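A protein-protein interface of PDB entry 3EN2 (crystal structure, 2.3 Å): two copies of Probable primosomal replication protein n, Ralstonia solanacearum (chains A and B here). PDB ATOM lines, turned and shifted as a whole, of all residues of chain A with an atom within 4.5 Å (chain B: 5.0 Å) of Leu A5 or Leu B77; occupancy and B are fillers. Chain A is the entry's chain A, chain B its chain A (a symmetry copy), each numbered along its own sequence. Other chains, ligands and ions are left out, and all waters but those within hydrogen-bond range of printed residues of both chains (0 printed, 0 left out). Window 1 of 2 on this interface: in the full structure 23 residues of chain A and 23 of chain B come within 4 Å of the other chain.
The backbone NH (N) of Gln A6 lies within hydrogen-bond range of the backbone carbonyl oxygen (O) of Arg B4.
O of Gly B75 sits at hydrogen-bond distance from N of Leu B5 (2.8 Å).
ND2 of Asn A3 is in hydrogen-bond range of O of Leu A77 (2.9 Å).
N of Leu A5 sits at hydrogen-bond distance from O of Gly A75, at 2.8 Å.
N of Cys A73 is in hydrogen-bond range of O of Leu A7 (2.8 Å).
The side-chain amide nitrogen of Asn B3 is in hydrogen-bond range of the backbone carbonyl oxygen of Leu B77, at 2.9 Å.
O of Arg A4 touches O of Arg B4, at 3.5 Å.
Arg B4 touches Leu A5 (O to CA, 3.4 Å).
Leu B77 touches Leu A5 (CD1 to CD2, 3.95 Å).
O of Gln A6 touches CA of Asn B3 (3.4 Å).
Leu A7 touches Asn B3 (CD1 to OD1, 3.8 Å).
CG1 of Val A46 touches O of Leu B77, 3.6 Å away.
Asn B3 touches Phe A48.
Phe A48 touches Leu B77 (CE2 to O, 3.3 Å).
CD1 of Phe A48 touches CD2 of Leu B87, at 3.8 Å.
Leu B87 touches Ile A50 (CD1 to CD1, 3.997 Å).
Of chain B, only Arg B4 and Leu B77 come within 4 Å of Leu A5.
Of chain A, only Leu A5 (3.95 Å), Val A46 (3.6 Å) and Phe A48 (3.3 Å) come within 4 Å of Leu B77.
Of the printed residues of chain A, Asn B3 touches Gln A6, Leu A7 and Phe A48.
Of the printed residues of chain A, Leu B87 touches Phe A48 (3.8 Å) and Ile A50 (3.997 Å).
Of the printed residues of chain B, Ile A50 touches Leu B87.
Asn A3 touches none of the printed residues of chain B.
The nearest residue of chain B that does not touch Leu A5 is Leu B5 (4.1 Å).
The nearest residue of chain A that does not touch Leu B77 is Ile A50 (4.1 Å).
The nearest printed residue of chain A that does not touch Asn B3 is Val A46 (4.2 Å).
Of the 13 printed residues of chain B, 5 touch a printed residue of chain A.
Hydrophobic or aromatic side chains of chain B within 4 Å of the printed part of chain A: Leu B5, Leu B77 and Leu B87.
Along chain B the printed residues that touch a printed residue of chain A span positions 3 to 87.
Among the printed residues, no Asp or Glu carboxylate lies within 4 Å of a Lys or Arg side-chain nitrogen of the other chain.
Arg B4 touches its own counterpart, Arg A4.
Arg A4 touches Leu B5, and with the chains exchanged Leu A5 touches Arg B4.
Leu A5 touches Leu B77, and with the chains exchanged Leu A77 touches Leu B5.
Positions printed for both chains: 3, 4, 5, 50, 75, 77 and 89.
Of the 13 pairs that touch across the chains among the printed residues, 5 have their exchanged pair printed and touching as well.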
ATOM      1  N   ASN A   3     -12.835   8.549   7.693  1.00  0.00           N
ATOM      2  CA  ASN A   3     -13.169   9.495   8.753  1.00  0.00           C
ATOM      3  C   ASN A   3     -14.658   9.275   8.934  1.00  0.00           C
ATOM      4  O   ASN A   3     -15.482   9.952   8.319  1.00  0.00           O
ATOM      5  CB  ASN A   3     -12.878  10.926   8.300  1.00  0.00           C
ATOM      6  CG  ASN A   3     -13.544  11.972   9.180  1.00  0.00           C
ATOM      7  OD1 ASN A   3     -13.896  11.709  10.327  1.00  0.00           O
ATOM      8  ND2 ASN A   3     -13.705  13.173   8.645  1.00  0.00           N
ATOM      9  N   ARG A   4     -14.998   8.300   9.768  1.00  0.00           N
ATOM     10  CA  ARG A   4     -16.390   7.953   9.988  1.00  0.00           C
ATOM     11  C   ARG A   4     -16.757   7.802  11.455  1.00  0.00           C
ATOM     12  O   ARG A   4     -16.139   7.030  12.193  1.00  0.00           O
ATOM     13  CB  ARG A   4     -16.699   6.660   9.230  1.00  0.00           C
ATOM     14  CG  ARG A   4     -18.139   6.186   9.305  1.00  0.00           C
ATOM     15  CD  ARG A   4     -18.525   5.507   7.996  1.00  0.00           C
ATOM     16  NE  ARG A   4     -19.862   4.921   8.043  1.00  0.00           N
ATOM     17  CZ  ARG A   4     -20.137   3.731   8.567  1.00  0.00           C
ATOM     18  NH1 ARG A   4     -21.386   3.279   8.572  1.00  0.00           N
ATOM     19  NH2 ARG A   4     -19.161   2.981   9.071  1.00  0.00           N
ATOM     20  N   LEU A   5     -17.768   8.556  11.868  1.00  0.00           N
ATOM     21  CA  LEU A   5     -18.259   8.504  13.233  1.00  0.00           C
ATOM     22  C   LEU A   5     -19.694   7.962  13.239  1.00  0.00           C
ATOM     23  O   LEU A   5     -20.539   8.391  12.449  1.00  0.00           O
ATOM     24  CB  LEU A   5     -18.233   9.901  13.862  1.00  0.00           C
ATOM     25  CG  LEU A   5     -18.810  10.018  15.281  1.00  0.00           C
ATOM     26  CD1 LEU A   5     -18.023   9.140  16.238  1.00  0.00           C
ATOM     27  CD2 LEU A   5     -18.774  11.463  15.732  1.00  0.00           C
ATOM     28  N   GLN A   6     -19.938   6.994  14.117  1.00  0.00           N
ATOM     29  CA  GLN A   6     -21.250   6.386  14.293  1.00  0.00           C
ATOM     30  C   GLN A   6     -21.617   6.745  15.722  1.00  0.00           C
ATOM     31  O   GLN A   6     -20.888   6.402  16.653  1.00  0.00           O
ATOM     32  CB  GLN A   6     -21.165   4.874  14.164  1.00  0.00           C
ATOM     33  CG  GLN A   6     -20.928   4.363  12.768  1.00  0.00           C
ATOM     34  CD  GLN A   6     -20.651   2.878  12.768  1.00  0.00           C
ATOM     35  OE1 GLN A   6     -19.523   2.448  13.008  1.00  0.00           O
ATOM     36  NE2 GLN A   6     -21.690   2.083  12.535  1.00  0.00           N
ATOM     37  N   LEU A   7     -22.741   7.424  15.905  1.00  0.00           N
ATOM     38  CA  LEU A   7     -23.116   7.842  17.240  1.00  0.00           C
ATOM     39  C   LEU A   7     -24.619   7.843  17.462  1.00  0.00           C
ATOM     40  O   LEU A   7     -25.366   8.452  16.697  1.00  0.00           O
ATOM     41  CB  LEU A   7     -22.563   9.251  17.491  1.00  0.00           C
ATOM     42  CG  LEU A   7     -22.562   9.845  18.901  1.00  0.00           C
ATOM     43  CD1 LEU A   7     -21.487   9.168  19.735  1.00  0.00           C
ATOM     44  CD2 LEU A   7     -22.276  11.336  18.837  1.00  0.00           C
ATOM     45  N   VAL A  46     -19.368   6.410  29.585  1.00  0.00           N
ATOM     46  CA  VAL A  46     -18.965   7.580  28.814  1.00  0.00           C
ATOM     47  C   VAL A  46     -20.127   8.537  28.592  1.00  0.00           C
ATOM     48  O   VAL A  46     -21.215   8.129  28.173  1.00  0.00           O
ATOM     49  CB  VAL A  46     -18.405   7.170  27.431  1.00  0.00           C
ATOM     50  CG1 VAL A  46     -18.120   8.406  26.588  1.00  0.00           C
ATOM     51  CG2 VAL A  46     -17.141   6.341  27.609  1.00  0.00           C
ATOM     52  N   PHE A  48     -20.896  12.650  27.098  1.00  0.00           N
ATOM     53  CA  PHE A  48     -20.372  13.870  26.523  1.00  0.00           C
ATOM     54  C   PHE A  48     -21.375  14.423  25.540  1.00  0.00           C
ATOM     55  O   PHE A  48     -22.291  13.716  25.113  1.00  0.00           O
ATOM     56  CB  PHE A  48     -19.034  13.607  25.813  1.00  0.00           C
ATOM     57  CG  PHE A  48     -19.158  12.812  24.537  1.00  0.00           C
ATOM     58  CD1 PHE A  48     -19.450  13.443  23.330  1.00  0.00           C
ATOM     59  CD2 PHE A  48     -18.964  11.433  24.536  1.00  0.00           C
ATOM     60  CE1 PHE A  48     -19.548  12.711  22.139  1.00  0.00           C
ATOM     61  CE2 PHE A  48     -19.062  10.694  23.348  1.00  0.00           C
ATOM     62  CZ  PHE A  48     -19.353  11.334  22.149  1.00  0.00           C
ATOM     63  N   ILE A  50     -21.651  16.909  21.901  1.00  0.00           N
ATOM     64  CA  ILE A  50     -20.835  17.282  20.762  1.00  0.00           C
ATOM     65  C   ILE A  50     -21.639  18.093  19.752  1.00  0.00           C
ATOM     66  O   ILE A  50     -22.789  17.767  19.463  1.00  0.00           O
ATOM     67  CB  ILE A  50     -20.276  16.016  20.084  1.00  0.00           C
ATOM     68  CG1 ILE A  50     -19.472  16.382  18.844  1.00  0.00           C
ATOM     69  CG2 ILE A  50     -21.421  15.088  19.696  1.00  0.00           C
ATOM     70  CD1 ILE A  50     -18.780  15.180  18.228  1.00  0.00           C
ATOM     71  N   CYS A  73     -26.849   8.264  14.365  1.00  0.00           N
ATOM     72  CA  CYS A  73     -26.131   9.043  13.368  1.00  0.00           C
ATOM     73  C   CYS A  73     -24.869   8.409  12.806  1.00  0.00           C
ATOM     74  O   CYS A  73     -24.186   7.619  13.471  1.00  0.00           O
ATOM     75  CB  CYS A  73     -25.732  10.397  13.951  1.00  0.00           C
ATOM     76  SG  CYS A  73     -26.978  11.222  14.939  1.00  0.00           S
ATOM     77  N   VAL A  74     -24.564   8.795  11.573  1.00  0.00           N
ATOM     78  CA  VAL A  74     -23.372   8.352  10.895  1.00  0.00           C
ATOM     79  C   VAL A  74     -22.886   9.598  10.167  1.00  0.00           C
ATOM     80  O   VAL A  74     -23.689  10.389   9.678  1.00  0.00           O
ATOM     81  CB  VAL A  74     -23.669   7.231   9.880  1.00  0.00           C
ATOM     82  CG1 VAL A  74     -24.431   7.783   8.686  1.00  0.00           C
ATOM     83  CG2 VAL A  74     -22.374   6.590   9.433  1.00  0.00           C
ATOM     84  N   GLY A  75     -21.576   9.795  10.116  1.00  0.00           N
ATOM     85  CA  GLY A  75     -21.060  10.963   9.439  1.00  0.00           C
ATOM     86  C   GLY A  75     -19.559  11.069   9.561  1.00  0.00           C
ATOM     87  O   GLY A  75     -18.871  10.061   9.729  1.00  0.00           O
ATOM     88  N   LEU A  77     -16.108  13.879  10.909  1.00  0.00           N
ATOM     89  CA  LEU A  77     -15.686  15.005  11.729  1.00  0.00           C
ATOM     90  C   LEU A  77     -15.018  16.053  10.851  1.00  0.00           C
ATOM     91  O   LEU A  77     -14.428  15.721   9.828  1.00  0.00           O
ATOM     92  CB  LEU A  77     -14.689  14.543  12.798  1.00  0.00           C
ATOM     93  CG  LEU A  77     -15.233  13.702  13.958  1.00  0.00           C
ATOM     94  CD1 LEU A  77     -14.106  13.355  14.927  1.00  0.00           C
ATOM     95  CD2 LEU A  77     -16.321  14.490  14.684  1.00  0.00           C
ATOM     96  N   PHE A  89     -19.495  17.554  14.238  1.00  0.00           N
ATOM     97  CA  PHE A  89     -19.906  16.274  13.678  1.00  0.00           C
ATOM     98  C   PHE A  89     -20.853  16.489  12.495  1.00  0.00           C
ATOM     99  O   PHE A  89     -21.991  16.928  12.671  1.00  0.00           O
ATOM    100  CB  PHE A  89     -20.590  15.452  14.788  1.00  0.00           C
ATOM    101  CG  PHE A  89     -21.174  14.130  14.330  1.00  0.00           C
ATOM    102  CD1 PHE A  89     -20.636  13.429  13.258  1.00  0.00           C
ATOM    103  CD2 PHE A  89     -22.231  13.555  15.034  1.00  0.00           C
ATOM    104  CE1 PHE A  89     -21.146  12.171  12.894  1.00  0.00           C
ATOM    105  CE2 PHE A  89     -22.743  12.305  14.679  1.00  0.00           C
ATOM    106  CZ  PHE A  89     -22.198  11.613  13.608  1.00  0.00           C
ATOM    107  N   ASN B   3     -20.769   4.382  19.757  1.00  0.00           N
ATOM    108  CA  ASN B   3     -19.899   5.554  19.781  1.00  0.00           C
ATOM    109  C   ASN B   3     -18.602   5.014  19.211  1.00  0.00           C
ATOM    110  O   ASN B   3     -17.720   4.570  19.944  1.00  0.00           O
ATOM    111  CB  ASN B   3     -19.705   6.043  21.216  1.00  0.00           C
ATOM    112  CG  ASN B   3     -18.532   7.001  21.361  1.00  0.00           C
ATOM    113  OD1 ASN B   3     -18.090   7.618  20.396  1.00  0.00           O
ATOM    114  ND2 ASN B   3     -18.034   7.138  22.580  1.00  0.00           N
ATOM    115  N   ARG B   4     -18.504   5.032  17.887  1.00  0.00           N
ATOM    116  CA  ARG B   4     -17.335   4.495  17.215  1.00  0.00           C
ATOM    117  C   ARG B   4     -16.776   5.410  16.139  1.00  0.00           C
ATOM    118  O   ARG B   4     -17.484   5.822  15.217  1.00  0.00           O
ATOM    119  CB  ARG B   4     -17.698   3.134  16.615  1.00  0.00           C
ATOM    120  CG  ARG B   4     -16.563   2.402  15.923  1.00  0.00           C
ATOM    121  CD  ARG B   4     -16.728   0.899  16.116  1.00  0.00           C
ATOM    122  NE  ARG B   4     -15.734   0.127  15.374  1.00  0.00           N
ATOM    123  CZ  ARG B   4     -15.837  -0.179  14.084  1.00  0.00           C
ATOM    124  NH1 ARG B   4     -14.880  -0.881  13.489  1.00  0.00           N
ATOM    125  NH2 ARG B   4     -16.906   0.201  13.392  1.00  0.00           N
ATOM    126  N   LEU B   5     -15.494   5.727  16.274  1.00  0.00           N
ATOM    127  CA  LEU B   5     -14.803   6.567  15.312  1.00  0.00           C
ATOM    128  C   LEU B   5     -13.713   5.749  14.610  1.00  0.00           C
ATOM    129  O   LEU B   5     -12.939   5.035  15.254  1.00  0.00           O
ATOM    130  CB  LEU B   5     -14.172   7.773  16.015  1.00  0.00           C
ATOM    131  CG  LEU B   5     -13.329   8.708  15.134  1.00  0.00           C
ATOM    132  CD1 LEU B   5     -14.188   9.300  14.030  1.00  0.00           C
ATOM    133  CD2 LEU B   5     -12.722   9.805  15.984  1.00  0.00           C
ATOM    134  N   ILE B  50      -6.843  16.240  15.892  1.00  0.00           N
ATOM    135  CA  ILE B  50      -7.660  15.862  17.029  1.00  0.00           C
ATOM    136  C   ILE B  50      -6.821  15.188  18.109  1.00  0.00           C
ATOM    137  O   ILE B  50      -5.963  14.361  17.809  1.00  0.00           O
ATOM    138  CB  ILE B  50      -8.780  14.908  16.572  1.00  0.00           C
ATOM    139  CG1 ILE B  50      -9.609  14.444  17.761  1.00  0.00           C
ATOM    140  CG2 ILE B  50      -8.175  13.699  15.866  1.00  0.00           C
ATOM    141  CD1 ILE B  50     -10.812  13.620  17.341  1.00  0.00           C
ATOM    142  N   GLY B  75     -11.922   3.553  17.548  1.00  0.00           N
ATOM    143  CA  GLY B  75     -12.075   3.822  18.959  1.00  0.00           C
ATOM    144  C   GLY B  75     -13.367   4.542  19.260  1.00  0.00           C
ATOM    145  O   GLY B  75     -14.340   4.421  18.514  1.00  0.00           O
ATOM    146  N   PHE B  76     -13.371   5.293  20.357  1.00  0.00           N
ATOM    147  CA  PHE B  76     -14.550   6.033  20.775  1.00  0.00           C
ATOM    148  C   PHE B  76     -14.175   7.426  21.274  1.00  0.00           C
ATOM    149  O   PHE B  76     -13.032   7.678  21.631  1.00  0.00           O
ATOM    150  CB  PHE B  76     -15.282   5.255  21.875  1.00  0.00           C
ATOM    151  CG  PHE B  76     -14.452   5.003  23.121  1.00  0.00           C
ATOM    152  CD1 PHE B  76     -14.555   5.843  24.228  1.00  0.00           C
ATOM    153  CD2 PHE B  76     -13.588   3.917  23.192  1.00  0.00           C
ATOM    154  CE1 PHE B  76     -13.808   5.606  25.400  1.00  0.00           C
ATOM    155  CE2 PHE B  76     -12.834   3.666  24.356  1.00  0.00           C
ATOM    156  CZ  PHE B  76     -12.953   4.515  25.454  1.00  0.00           C
ATOM    157  N   LEU B  77     -15.151   8.328  21.287  1.00  0.00           N
ATOM    158  CA  LEU B  77     -14.943   9.695  21.742  1.00  0.00           C
ATOM    159  C   LEU B  77     -15.319   9.805  23.213  1.00  0.00           C
ATOM    160  O   LEU B  77     -16.177   9.071  23.690  1.00  0.00           O
ATOM    161  CB  LEU B  77     -15.811  10.665  20.933  1.00  0.00           C
ATOM    162  CG  LEU B  77     -15.415  10.925  19.476  1.00  0.00           C
ATOM    163  CD1 LEU B  77     -16.376  11.926  18.841  1.00  0.00           C
ATOM    164  CD2 LEU B  77     -13.989  11.471  19.432  1.00  0.00           C
ATOM    165  N   ALA B  78     -14.672  10.713  23.932  1.00  0.00           N
ATOM    166  CA  ALA B  78     -14.986  10.908  25.339  1.00  0.00           C
ATOM    167  C   ALA B  78     -14.606  12.318  25.778  1.00  0.00           C
ATOM    168  O   ALA B  78     -13.946  13.050  25.044  1.00  0.00           O
ATOM    169  CB  ALA B  78     -14.259   9.876  26.186  1.00  0.00           C
ATOM    170  N   ARG B  79     -15.045  12.704  26.968  1.00  0.00           N
ATOM    171  CA  ARG B  79     -14.721  14.023  27.485  1.00  0.00           C
ATOM    172  C   ARG B  79     -13.306  13.950  28.053  1.00  0.00           C
ATOM    173  O   ARG B  79     -12.957  12.986  28.737  1.00  0.00           O
ATOM    174  CB  ARG B  79     -15.721  14.423  28.574  1.00  0.00           C
ATOM    175  CG  ARG B  79     -15.463  15.789  29.178  1.00  0.00           C
ATOM    176  CD  ARG B  79     -16.540  16.166  30.179  1.00  0.00           C
ATOM    177  NE  ARG B  79     -17.869  16.169  29.573  1.00  0.00           N
ATOM    178  CZ  ARG B  79     -18.965  16.608  30.185  1.00  0.00           C
ATOM    179  NH1 ARG B  79     -18.885  17.084  31.424  1.00  0.00           N
ATOM    180  NH2 ARG B  79     -20.138  16.572  29.562  1.00  0.00           N
ATOM    181  N   LEU B  87     -13.015  17.229  23.803  1.00  0.00           N
ATOM    182  CA  LEU B  87     -13.156  15.798  23.562  1.00  0.00           C
ATOM    183  C   LEU B  87     -11.820  15.197  23.157  1.00  0.00           C
ATOM    184  O   LEU B  87     -10.963  15.884  22.610  1.00  0.00           O
ATOM    185  CB  LEU B  87     -14.180  15.536  22.451  1.00  0.00           C
ATOM    186  CG  LEU B  87     -15.609  16.047  22.647  1.00  0.00           C
ATOM    187  CD1 LEU B  87     -16.424  15.701  21.414  1.00  0.00           C
ATOM    188  CD2 LEU B  87     -16.229  15.437  23.901  1.00  0.00           C
ATOM    189  N   VAL B  88     -11.654  13.910  23.427  1.00  0.00           N
ATOM    190  CA  VAL B  88     -10.436  13.214  23.084  1.00  0.00           C
ATOM    191  C   VAL B  88     -10.818  11.895  22.441  1.00  0.00           C
ATOM    192  O   VAL B  88     -11.810  11.289  22.824  1.00  0.00           O
ATOM    193  CB  VAL B  88      -9.562  12.970  24.342  1.00  0.00           C
ATOM    194  CG1 VAL B  88     -10.340  12.189  25.372  1.00  0.00           C
ATOM    195  CG2 VAL B  88      -8.291  12.242  23.961  1.00  0.00           C
ATOM    196  N   PHE B  89     -10.039  11.476  21.448  1.00  0.00           N
ATOM    197  CA  PHE B  89     -10.265  10.235  20.719  1.00  0.00           C
ATOM    198  C   PHE B  89      -9.559   9.070  21.416  1.00  0.00           C
ATOM    199  O   PHE B  89      -8.329   8.996  21.426  1.00  0.00           O
ATOM    200  CB  PHE B  89      -9.745  10.413  19.279  1.00  0.00           C
ATOM    201  CG  PHE B  89      -9.810   9.165  18.422  1.00  0.00           C
ATOM    202  CD1 PHE B  89     -10.773   8.185  18.635  1.00  0.00           C
ATOM    203  CD2 PHE B  89      -8.937   9.012  17.346  1.00  0.00           C
ATOM    204  CE1 PHE B  89     -10.863   7.070  17.784  1.00  0.00           C
ATOM    205  CE2 PHE B  89      -9.020   7.907  16.496  1.00  0.00           C
ATOM    206  CZ  PHE B  89      -9.986   6.936  16.716  1.00  0.00           C
ATOM    207  N   HIS B  90     -10.334   8.173  22.016  1.00  0.00           N
ATOM    208  CA  HIS B  90      -9.758   7.013  22.689  1.00  0.00           C
ATOM    209  C   HIS B  90      -9.562   5.911  21.647  1.00  0.00           C
ATOM    210  O   HIS B  90     -10.535   5.400  21.081  1.00  0.00           O
ATOM    211  CB  HIS B  90     -10.694   6.515  23.796  1.00  0.00           C
ATOM    212  CG  HIS B  90     -10.703   7.375  25.022  1.00  0.00           C
ATOM    213  ND1 HIS B  90     -10.419   6.877  26.274  1.00  0.00           N
ATOM    214  CD2 HIS B  90     -10.975   8.691  25.195  1.00  0.00           C
ATOM    215  CE1 HIS B  90     -10.515   7.847  27.166  1.00  0.00           C
ATOM    216  NE2 HIS B  90     -10.850   8.958  26.537  1.00  0.00           N
